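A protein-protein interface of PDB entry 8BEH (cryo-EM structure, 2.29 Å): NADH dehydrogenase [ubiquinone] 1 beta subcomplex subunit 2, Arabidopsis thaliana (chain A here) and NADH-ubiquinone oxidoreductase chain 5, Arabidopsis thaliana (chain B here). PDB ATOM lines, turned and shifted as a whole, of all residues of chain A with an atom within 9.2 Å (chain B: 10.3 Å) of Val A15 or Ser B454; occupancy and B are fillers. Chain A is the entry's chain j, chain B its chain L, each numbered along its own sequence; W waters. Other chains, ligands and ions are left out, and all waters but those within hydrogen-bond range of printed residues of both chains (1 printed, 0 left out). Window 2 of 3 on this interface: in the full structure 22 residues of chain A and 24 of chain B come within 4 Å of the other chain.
The side-chain hydroxyl (OG) of Ser B454 sits at hydrogen-bond distance from the backbone carbonyl oxygen (O) of Thr A16, at 2.8 Å.
O of Ser B454 sits at hydrogen-bond distance from NE2 of His A18 (2.8 Å).
The backbone carbonyl oxygen (O) of Ala B358 sits close to the side-chain sulfur (SG) of Cys B456 (3.8 Å).
SG of Cys B456 is in hydrogen-bond range of SD of Met B359 (3.5 Å).
O of Asp B452 lies within hydrogen-bond range of SG of Cys B456 (3.0 Å).
The side-chain sulfur (SG) of Cys B456 is in hydrogen-bond range of the backbone carbonyl oxygen (O) of Ile B453, at 3.1 Å.
N of Ile A10 is in hydrogen-bond range of O of Val A17, 3.0 Å away.
The side-chain hydroxyl (OG1) of Thr A16 is in hydrogen-bond range of the side-chain hydroxyl (OG1) of Thr A11 (2.4 Å).
Among the printed residues, pairs that only touch across the chains: Val A15 with Ile B453 (3.6 Å), Val A15 with Ser B454 (3.6 Å), Val A17 with Ile B453 (3.7 Å), His A18 with Cys B456 (3.7 Å) and Thr A16 with Ile B453 (3.96 Å).
No residue of chain B comes within 4 Å of Thr A11.
No residue of chain B comes within 4 Å of Gly A14.
Of the printed residues of chain B, Val A15 touches Ile B453 (3.6 Å) and Ser B454 (3.6 Å).
Of chain B, only Ile B453 and Ser B454 come within 4 Å of Thr A16.
Of the printed residues of chain B, Val A17 touches Ile B453 (3.7 Å).
Of the printed residues of chain B, His A18 touches Ser B454 (2.8 Å) and Cys B456 (3.7 Å).
Ser B360 touches none of the printed residues of chain A.
Ser B448 touches none of the printed residues of chain A.
Of the printed residues of chain A, Ile B453 touches Val A15, Thr A16 and Val A17.
Ser B454 touches just these residues of chain A: Val A15 (3.6 Å), Thr A16 (2.8 Å) and His A18 (2.8 Å).
Of the printed residues of chain A, Cys B456 touches His A18 (3.7 Å).
The nearest residue of chain A that does not touch Ser B454 is Gly A14 (4.6 Å).
The nearest printed residue of chain A that does not touch Ile B453 is His A18 (4.5 Å).
Hydrophobic or aromatic side chains of chain B within 4 Å of the printed part of chain A: Ile B453.
Among the printed residues, no Asp or Glu carboxylate lies within 4 Å of a Lys or Arg side-chain nitrogen of the other chain.
Water W1 lies within hydrogen-bond range of the backbone carbonyl oxygen (O) of Ile B453 (3.4 Å), the backbone NH (N) of His A18 (3.4 Å) and the backbone carbonyl oxygen (O) of Cys B456 (3.4 Å).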
ATOM      1  N   GLY A   9     -22.149 -18.255 -28.691  1.00  0.00           N
ATOM      2  CA  GLY A   9     -21.553 -18.356 -27.373  1.00  0.00           C
ATOM      3  C   GLY A   9     -20.209 -17.666 -27.219  1.00  0.00           C
ATOM      4  O   GLY A   9     -19.571 -17.296 -28.205  1.00  0.00           O
ATOM      5  N   ILE A  10     -19.780 -17.496 -25.969  1.00  0.00           N
ATOM      6  CA  ILE A  10     -18.510 -16.860 -25.639  1.00  0.00           C
ATOM      7  C   ILE A  10     -17.578 -17.907 -25.048  1.00  0.00           C
ATOM      8  O   ILE A  10     -17.954 -18.633 -24.118  1.00  0.00           O
ATOM      9  CB  ILE A  10     -18.714 -15.687 -24.665  1.00  0.00           C
ATOM     10  CG1 ILE A  10     -19.725 -14.695 -25.245  1.00  0.00           C
ATOM     11  CG2 ILE A  10     -17.394 -14.989 -24.381  1.00  0.00           C
ATOM     12  CD1 ILE A  10     -20.865 -14.374 -24.317  1.00  0.00           C
ATOM     13  N   THR A  11     -16.363 -17.991 -25.584  1.00  0.00           N
ATOM     14  CA  THR A  11     -15.401 -19.020 -25.209  1.00  0.00           C
ATOM     15  C   THR A  11     -14.309 -18.394 -24.352  1.00  0.00           C
ATOM     16  O   THR A  11     -13.632 -17.459 -24.789  1.00  0.00           O
ATOM     17  CB  THR A  11     -14.798 -19.680 -26.446  1.00  0.00           C
ATOM     18  OG1 THR A  11     -15.837 -20.301 -27.212  1.00  0.00           O
ATOM     19  CG2 THR A  11     -13.782 -20.735 -26.041  1.00  0.00           C
ATOM     20  N   TYR A  12     -14.137 -18.916 -23.140  1.00  0.00           N
ATOM     21  CA  TYR A  12     -13.122 -18.443 -22.204  1.00  0.00           C
ATOM     22  C   TYR A  12     -12.265 -19.627 -21.780  1.00  0.00           C
ATOM     23  O   TYR A  12     -12.730 -20.496 -21.034  1.00  0.00           O
ATOM     24  CB  TYR A  12     -13.758 -17.776 -20.987  1.00  0.00           C
ATOM     25  CG  TYR A  12     -12.808 -16.924 -20.185  1.00  0.00           C
ATOM     26  CD1 TYR A  12     -11.542 -16.622 -20.659  1.00  0.00           C
ATOM     27  CD2 TYR A  12     -13.163 -16.460 -18.930  1.00  0.00           C
ATOM     28  CE1 TYR A  12     -10.670 -15.852 -19.920  1.00  0.00           C
ATOM     29  CE2 TYR A  12     -12.298 -15.694 -18.181  1.00  0.00           C
ATOM     30  CZ  TYR A  12     -11.053 -15.390 -18.680  1.00  0.00           C
ATOM     31  OH  TYR A  12     -10.189 -14.626 -17.933  1.00  0.00           O
ATOM     32  N   LYS A  13     -11.013 -19.641 -22.246  1.00  0.00           N
ATOM     33  CA  LYS A  13     -10.022 -20.680 -21.973  1.00  0.00           C
ATOM     34  C   LYS A  13     -10.616 -22.085 -21.961  1.00  0.00           C
ATOM     35  O   LYS A  13     -10.599 -22.772 -20.934  1.00  0.00           O
ATOM     36  CB  LYS A  13      -9.249 -20.403 -20.670  1.00  0.00           C
ATOM     37  CG  LYS A  13     -10.037 -20.019 -19.435  1.00  0.00           C
ATOM     38  CD  LYS A  13      -9.101 -19.885 -18.248  1.00  0.00           C
ATOM     39  CE  LYS A  13      -8.718 -18.445 -17.950  1.00  0.00           C
ATOM     40  NZ  LYS A  13      -9.776 -17.714 -17.205  1.00  0.00           N
ATOM     41  N   GLY A  14     -11.127 -22.517 -23.098  1.00  0.00           N
ATOM     42  CA  GLY A  14     -11.649 -23.869 -23.252  1.00  0.00           C
ATOM     43  C   GLY A  14     -13.135 -24.030 -23.086  1.00  0.00           C
ATOM     44  O   GLY A  14     -13.787 -24.674 -23.906  1.00  0.00           O
ATOM     45  N   VAL A  15     -13.690 -23.459 -22.028  1.00  0.00           N
ATOM     46  CA  VAL A  15     -15.107 -23.614 -21.736  1.00  0.00           C
ATOM     47  C   VAL A  15     -15.907 -22.607 -22.552  1.00  0.00           C
ATOM     48  O   VAL A  15     -15.615 -21.407 -22.548  1.00  0.00           O
ATOM     49  CB  VAL A  15     -15.367 -23.459 -20.231  1.00  0.00           C
ATOM     50  CG1 VAL A  15     -16.845 -23.475 -19.952  1.00  0.00           C
ATOM     51  CG2 VAL A  15     -14.661 -24.571 -19.468  1.00  0.00           C
ATOM     52  N   THR A  16     -16.922 -23.098 -23.255  1.00  0.00           N
ATOM     53  CA  THR A  16     -17.791 -22.275 -24.080  1.00  0.00           C
ATOM     54  C   THR A  16     -19.189 -22.266 -23.481  1.00  0.00           C
ATOM     55  O   THR A  16     -19.769 -23.328 -23.231  1.00  0.00           O
ATOM     56  CB  THR A  16     -17.834 -22.797 -25.517  1.00  0.00           C
ATOM     57  OG1 THR A  16     -16.686 -22.323 -26.231  1.00  0.00           O
ATOM     58  CG2 THR A  16     -19.089 -22.324 -26.225  1.00  0.00           C
ATOM     59  N   VAL A  17     -19.728 -21.074 -23.250  1.00  0.00           N
ATOM     60  CA  VAL A  17     -21.065 -20.912 -22.692  1.00  0.00           C
ATOM     61  C   VAL A  17     -21.949 -20.288 -23.760  1.00  0.00           C
ATOM     62  O   VAL A  17     -21.611 -19.239 -24.319  1.00  0.00           O
ATOM     63  CB  VAL A  17     -21.049 -20.061 -21.412  1.00  0.00           C
ATOM     64  CG1 VAL A  17     -22.354 -20.232 -20.647  1.00  0.00           C
ATOM     65  CG2 VAL A  17     -19.867 -20.431 -20.544  1.00  0.00           C
ATOM     66  N   HIS A  18     -23.066 -20.945 -24.054  1.00  0.00           N
ATOM     67  CA  HIS A  18     -24.006 -20.472 -25.058  1.00  0.00           C
ATOM     68  C   HIS A  18     -24.983 -19.478 -24.452  1.00  0.00           C
ATOM     69  O   HIS A  18     -25.521 -19.700 -23.364  1.00  0.00           O
ATOM     70  CB  HIS A  18     -24.781 -21.636 -25.677  1.00  0.00           C
ATOM     71  CG  HIS A  18     -23.948 -22.849 -25.946  1.00  0.00           C
ATOM     72  ND1 HIS A  18     -23.234 -23.014 -27.112  1.00  0.00           N
ATOM     73  CD2 HIS A  18     -23.728 -23.964 -25.209  1.00  0.00           C
ATOM     74  CE1 HIS A  18     -22.603 -24.173 -27.080  1.00  0.00           C
ATOM     75  NE2 HIS A  18     -22.884 -24.768 -25.935  1.00  0.00           N
ATOM     76  N   ALA B 358     -30.690 -30.206 -18.860  1.00  0.00           N
ATOM     77  CA  ALA B 358     -29.717 -29.263 -19.394  1.00  0.00           C
ATOM     78  C   ALA B 358     -28.297 -29.560 -18.930  1.00  0.00           C
ATOM     79  O   ALA B 358     -27.344 -29.188 -19.618  1.00  0.00           O
ATOM     80  CB  ALA B 358     -30.103 -27.837 -18.998  1.00  0.00           C
ATOM     81  N   MET B 359     -28.133 -30.219 -17.785  1.00  0.00           N
ATOM     82  CA  MET B 359     -26.827 -30.485 -17.201  1.00  0.00           C
ATOM     83  C   MET B 359     -26.360 -31.916 -17.448  1.00  0.00           C
ATOM     84  O   MET B 359     -25.584 -32.458 -16.656  1.00  0.00           O
ATOM     85  CB  MET B 359     -26.857 -30.184 -15.705  1.00  0.00           C
ATOM     86  CG  MET B 359     -26.905 -28.708 -15.362  1.00  0.00           C
ATOM     87  SD  MET B 359     -25.818 -27.711 -16.383  1.00  0.00           S
ATOM     88  CE  MET B 359     -24.331 -27.762 -15.388  1.00  0.00           C
ATOM     89  N   SER B 360     -26.822 -32.510 -18.544  1.00  0.00           N
ATOM     90  CA  SER B 360     -26.469 -33.909 -18.961  1.00  0.00           C
ATOM     91  C   SER B 360     -26.772 -34.909 -17.862  1.00  0.00           C
ATOM     92  O   SER B 360     -25.905 -35.734 -17.590  1.00  0.00           O
ATOM     93  CB  SER B 360     -25.049 -33.943 -19.426  1.00  0.00           C
ATOM     94  OG  SER B 360     -24.716 -32.796 -20.172  1.00  0.00           O
ATOM     95  N   GLY B 370     -23.894 -21.081 -10.493  1.00  0.00           N
ATOM     96  CA  GLY B 370     -23.663 -20.110 -11.551  1.00  0.00           C
ATOM     97  C   GLY B 370     -24.495 -20.375 -12.784  1.00  0.00           C
ATOM     98  O   GLY B 370     -24.019 -20.183 -13.908  1.00  0.00           O
ATOM     99  N   LEU B 371     -25.734 -20.815 -12.598  1.00  0.00           N
ATOM    100  CA  LEU B 371     -26.591 -21.242 -13.691  1.00  0.00           C
ATOM    101  C   LEU B 371     -27.746 -20.285 -13.956  1.00  0.00           C
ATOM    102  O   LEU B 371     -28.517 -20.513 -14.892  1.00  0.00           O
ATOM    103  CB  LEU B 371     -27.130 -22.646 -13.392  1.00  0.00           C
ATOM    104  CG  LEU B 371     -26.502 -23.839 -14.111  1.00  0.00           C
ATOM    105  CD1 LEU B 371     -24.987 -23.770 -14.115  1.00  0.00           C
ATOM    106  CD2 LEU B 371     -26.971 -25.140 -13.469  1.00  0.00           C
ATOM    107  N   SER B 374     -27.421 -18.756 -17.469  1.00  0.00           N
ATOM    108  CA  SER B 374     -27.461 -19.724 -18.558  1.00  0.00           C
ATOM    109  C   SER B 374     -28.863 -20.272 -18.795  1.00  0.00           C
ATOM    110  O   SER B 374     -29.225 -20.553 -19.941  1.00  0.00           O
ATOM    111  CB  SER B 374     -26.486 -20.871 -18.281  1.00  0.00           C
ATOM    112  OG  SER B 374     -27.143 -21.973 -17.685  1.00  0.00           O
ATOM    113  N   PHE B 375     -29.662 -20.431 -17.741  1.00  0.00           N
ATOM    114  CA  PHE B 375     -31.039 -20.905 -17.847  1.00  0.00           C
ATOM    115  C   PHE B 375     -31.952 -19.885 -17.181  1.00  0.00           C
ATOM    116  O   PHE B 375     -32.432 -20.103 -16.060  1.00  0.00           O
ATOM    117  CB  PHE B 375     -31.221 -22.289 -17.225  1.00  0.00           C
ATOM    118  CG  PHE B 375     -30.110 -23.244 -17.527  1.00  0.00           C
ATOM    119  CD1 PHE B 375     -29.420 -23.870 -16.508  1.00  0.00           C
ATOM    120  CD2 PHE B 375     -29.759 -23.522 -18.836  1.00  0.00           C
ATOM    121  CE1 PHE B 375     -28.404 -24.760 -16.789  1.00  0.00           C
ATOM    122  CE2 PHE B 375     -28.742 -24.399 -19.119  1.00  0.00           C
ATOM    123  CZ  PHE B 375     -28.062 -25.020 -18.095  1.00  0.00           C
ATOM    124  N   THR B 446     -19.729 -21.233  -9.775  1.00  0.00           N
ATOM    125  CA  THR B 446     -20.050 -22.555 -10.296  1.00  0.00           C
ATOM    126  C   THR B 446     -19.098 -23.623  -9.766  1.00  0.00           C
ATOM    127  O   THR B 446     -17.881 -23.430  -9.698  1.00  0.00           O
ATOM    128  CB  THR B 446     -20.036 -22.546 -11.829  1.00  0.00           C
ATOM    129  OG1 THR B 446     -20.410 -23.839 -12.320  1.00  0.00           O
ATOM    130  CG2 THR B 446     -18.663 -22.187 -12.373  1.00  0.00           C
ATOM    131  N   SER B 448     -19.495 -26.778 -11.147  1.00  0.00           N
ATOM    132  CA  SER B 448     -19.811 -27.803 -12.123  1.00  0.00           C
ATOM    133  C   SER B 448     -18.581 -28.183 -12.944  1.00  0.00           C
ATOM    134  O   SER B 448     -17.500 -27.610 -12.812  1.00  0.00           O
ATOM    135  CB  SER B 448     -20.935 -27.330 -13.044  1.00  0.00           C
ATOM    136  OG  SER B 448     -20.517 -26.241 -13.835  1.00  0.00           O
ATOM    137  N   PHE B 449     -18.787 -29.102 -13.863  1.00  0.00           N
ATOM    138  CA  PHE B 449     -17.747 -29.587 -14.777  1.00  0.00           C
ATOM    139  C   PHE B 449     -17.854 -28.730 -16.044  1.00  0.00           C
ATOM    140  O   PHE B 449     -18.966 -28.411 -16.431  1.00  0.00           O
ATOM    141  CB  PHE B 449     -18.025 -31.086 -14.991  1.00  0.00           C
ATOM    142  CG  PHE B 449     -17.733 -32.002 -13.829  1.00  0.00           C
ATOM    143  CD1 PHE B 449     -18.735 -32.397 -12.961  1.00  0.00           C
ATOM    144  CD2 PHE B 449     -16.465 -32.523 -13.633  1.00  0.00           C
ATOM    145  CE1 PHE B 449     -18.478 -33.262 -11.910  1.00  0.00           C
ATOM    146  CE2 PHE B 449     -16.204 -33.386 -12.580  1.00  0.00           C
ATOM    147  CZ  PHE B 449     -17.211 -33.757 -11.720  1.00  0.00           C
ATOM    148  N   GLY B 450     -16.746 -28.320 -16.631  1.00  0.00           N
ATOM    149  CA  GLY B 450     -16.781 -27.593 -17.896  1.00  0.00           C
ATOM    150  C   GLY B 450     -17.527 -28.310 -18.984  1.00  0.00           C
ATOM    151  O   GLY B 450     -18.278 -27.633 -19.697  1.00  0.00           O
ATOM    152  N   ARG B 451     -17.401 -29.636 -19.071  1.00  0.00           N
ATOM    153  CA  ARG B 451     -18.067 -30.372 -20.179  1.00  0.00           C
ATOM    154  C   ARG B 451     -19.592 -30.231 -20.033  1.00  0.00           C
ATOM    155  O   ARG B 451     -20.282 -30.294 -21.066  1.00  0.00           O
ATOM    156  CB  ARG B 451     -17.610 -31.835 -20.240  1.00  0.00           C
ATOM    157  CG  ARG B 451     -18.222 -32.666 -21.359  1.00  0.00           C
ATOM    158  CD  ARG B 451     -17.716 -34.093 -21.463  1.00  0.00           C
ATOM    159  NE  ARG B 451     -18.050 -34.933 -20.321  1.00  0.00           N
ATOM    160  CZ  ARG B 451     -19.211 -35.557 -20.160  1.00  0.00           C
ATOM    161  NH1 ARG B 451     -20.165 -35.428 -21.066  1.00  0.00           N
ATOM    162  NH2 ARG B 451     -19.420 -36.297 -19.086  1.00  0.00           N
ATOM    163  N   ASP B 452     -20.092 -30.036 -18.805  1.00  0.00           N
ATOM    164  CA  ASP B 452     -21.551 -29.856 -18.608  1.00  0.00           C
ATOM    165  C   ASP B 452     -21.995 -28.452 -19.077  1.00  0.00           C
ATOM    166  O   ASP B 452     -22.914 -28.398 -19.823  1.00  0.00           O
ATOM    167  CB  ASP B 452     -21.975 -30.246 -17.177  1.00  0.00           C
ATOM    168  CG  ASP B 452     -21.858 -31.717 -16.847  1.00  0.00           C
ATOM    169  OD1 ASP B 452     -22.199 -32.546 -17.700  1.00  0.00           O
ATOM    170  OD2 ASP B 452     -21.440 -32.012 -15.737  1.00  0.00           O
ATOM    171  N   ILE B 453     -21.238 -27.415 -18.757  1.00  0.00           N
ATOM    172  CA  ILE B 453     -21.570 -25.986 -19.069  1.00  0.00           C
ATOM    173  C   ILE B 453     -21.580 -25.772 -20.568  1.00  0.00           C
ATOM    174  O   ILE B 453     -22.510 -25.194 -21.060  1.00  0.00           O
ATOM    175  CB  ILE B 453     -20.494 -25.153 -18.332  1.00  0.00           C
ATOM    176  CG1 ILE B 453     -20.825 -24.990 -16.850  1.00  0.00           C
ATOM    177  CG2 ILE B 453     -20.265 -23.811 -19.005  1.00  0.00           C
ATOM    178  CD1 ILE B 453     -22.256 -24.598 -16.601  1.00  0.00           C
ATOM    179  N   SER B 454     -20.696 -26.449 -21.266  1.00  0.00           N
ATOM    180  CA  SER B 454     -20.439 -26.287 -22.695  1.00  0.00           C
ATOM    181  C   SER B 454     -21.418 -27.081 -23.562  1.00  0.00           C
ATOM    182  O   SER B 454     -21.411 -26.878 -24.715  1.00  0.00           O
ATOM    183  CB  SER B 454     -18.987 -26.670 -22.846  1.00  0.00           C
ATOM    184  OG  SER B 454     -18.162 -25.556 -22.606  1.00  0.00           O
ATOM    185  N   ARG B 455     -22.343 -27.781 -22.949  1.00  0.00           N
ATOM    186  CA  ARG B 455     -23.353 -28.586 -23.647  1.00  0.00           C
ATOM    187  C   ARG B 455     -24.764 -28.214 -23.126  1.00  0.00           C
ATOM    188  O   ARG B 455     -25.668 -28.962 -23.446  1.00  0.00           O
ATOM    189  CB  ARG B 455     -23.009 -30.050 -23.420  1.00  0.00           C
ATOM    190  CG  ARG B 455     -21.711 -30.538 -24.035  1.00  0.00           C
ATOM    191  CD  ARG B 455     -21.566 -32.014 -23.735  1.00  0.00           C
ATOM    192  NE  ARG B 455     -21.883 -32.848 -24.879  1.00  0.00           N
ATOM    193  CZ  ARG B 455     -20.990 -33.548 -25.574  1.00  0.00           C
ATOM    194  NH1 ARG B 455     -19.715 -33.536 -25.223  1.00  0.00           N
ATOM    195  NH2 ARG B 455     -21.381 -34.271 -26.607  1.00  0.00           N
ATOM    196  N   CYS B 456     -24.982 -27.069 -22.460  1.00  0.00           N
ATOM    197  CA  CYS B 456     -26.259 -26.709 -21.864  1.00  0.00           C
ATOM    198  C   CYS B 456     -27.227 -26.140 -22.901  1.00  0.00           C
ATOM    199  O   CYS B 456     -26.832 -25.655 -23.964  1.00  0.00           O
ATOM    200  CB  CYS B 456     -26.051 -25.692 -20.747  1.00  0.00           C
ATOM    201  SG  CYS B 456     -24.970 -26.241 -19.418  1.00  0.00           S
ATOM    202  N   HIS B 457     -28.511 -26.189 -22.555  1.00  0.00           N
ATOM    203  CA  HIS B 457     -29.603 -25.703 -23.387  1.00  0.00           C
ATOM    204  C   HIS B 457     -30.843 -25.568 -22.516  1.00  0.00           C
ATOM    205  O   HIS B 457     -31.074 -26.398 -21.636  1.00  0.00           O
ATOM    206  CB  HIS B 457     -29.867 -26.659 -24.554  1.00  0.00           C
ATOM    207  CG  HIS B 457     -30.262 -28.037 -24.124  1.00  0.00           C
ATOM    208  ND1 HIS B 457     -29.386 -29.100 -24.139  1.00  0.00           N
ATOM    209  CD2 HIS B 457     -31.441 -28.529 -23.674  1.00  0.00           C
ATOM    210  CE1 HIS B 457     -30.005 -30.184 -23.706  1.00  0.00           C
ATOM    211  NE2 HIS B 457     -31.253 -29.864 -23.417  1.00  0.00           N
HETATM  212  O   HOH W   1     -24.898 -23.285 -22.472  1.00  0.00           O
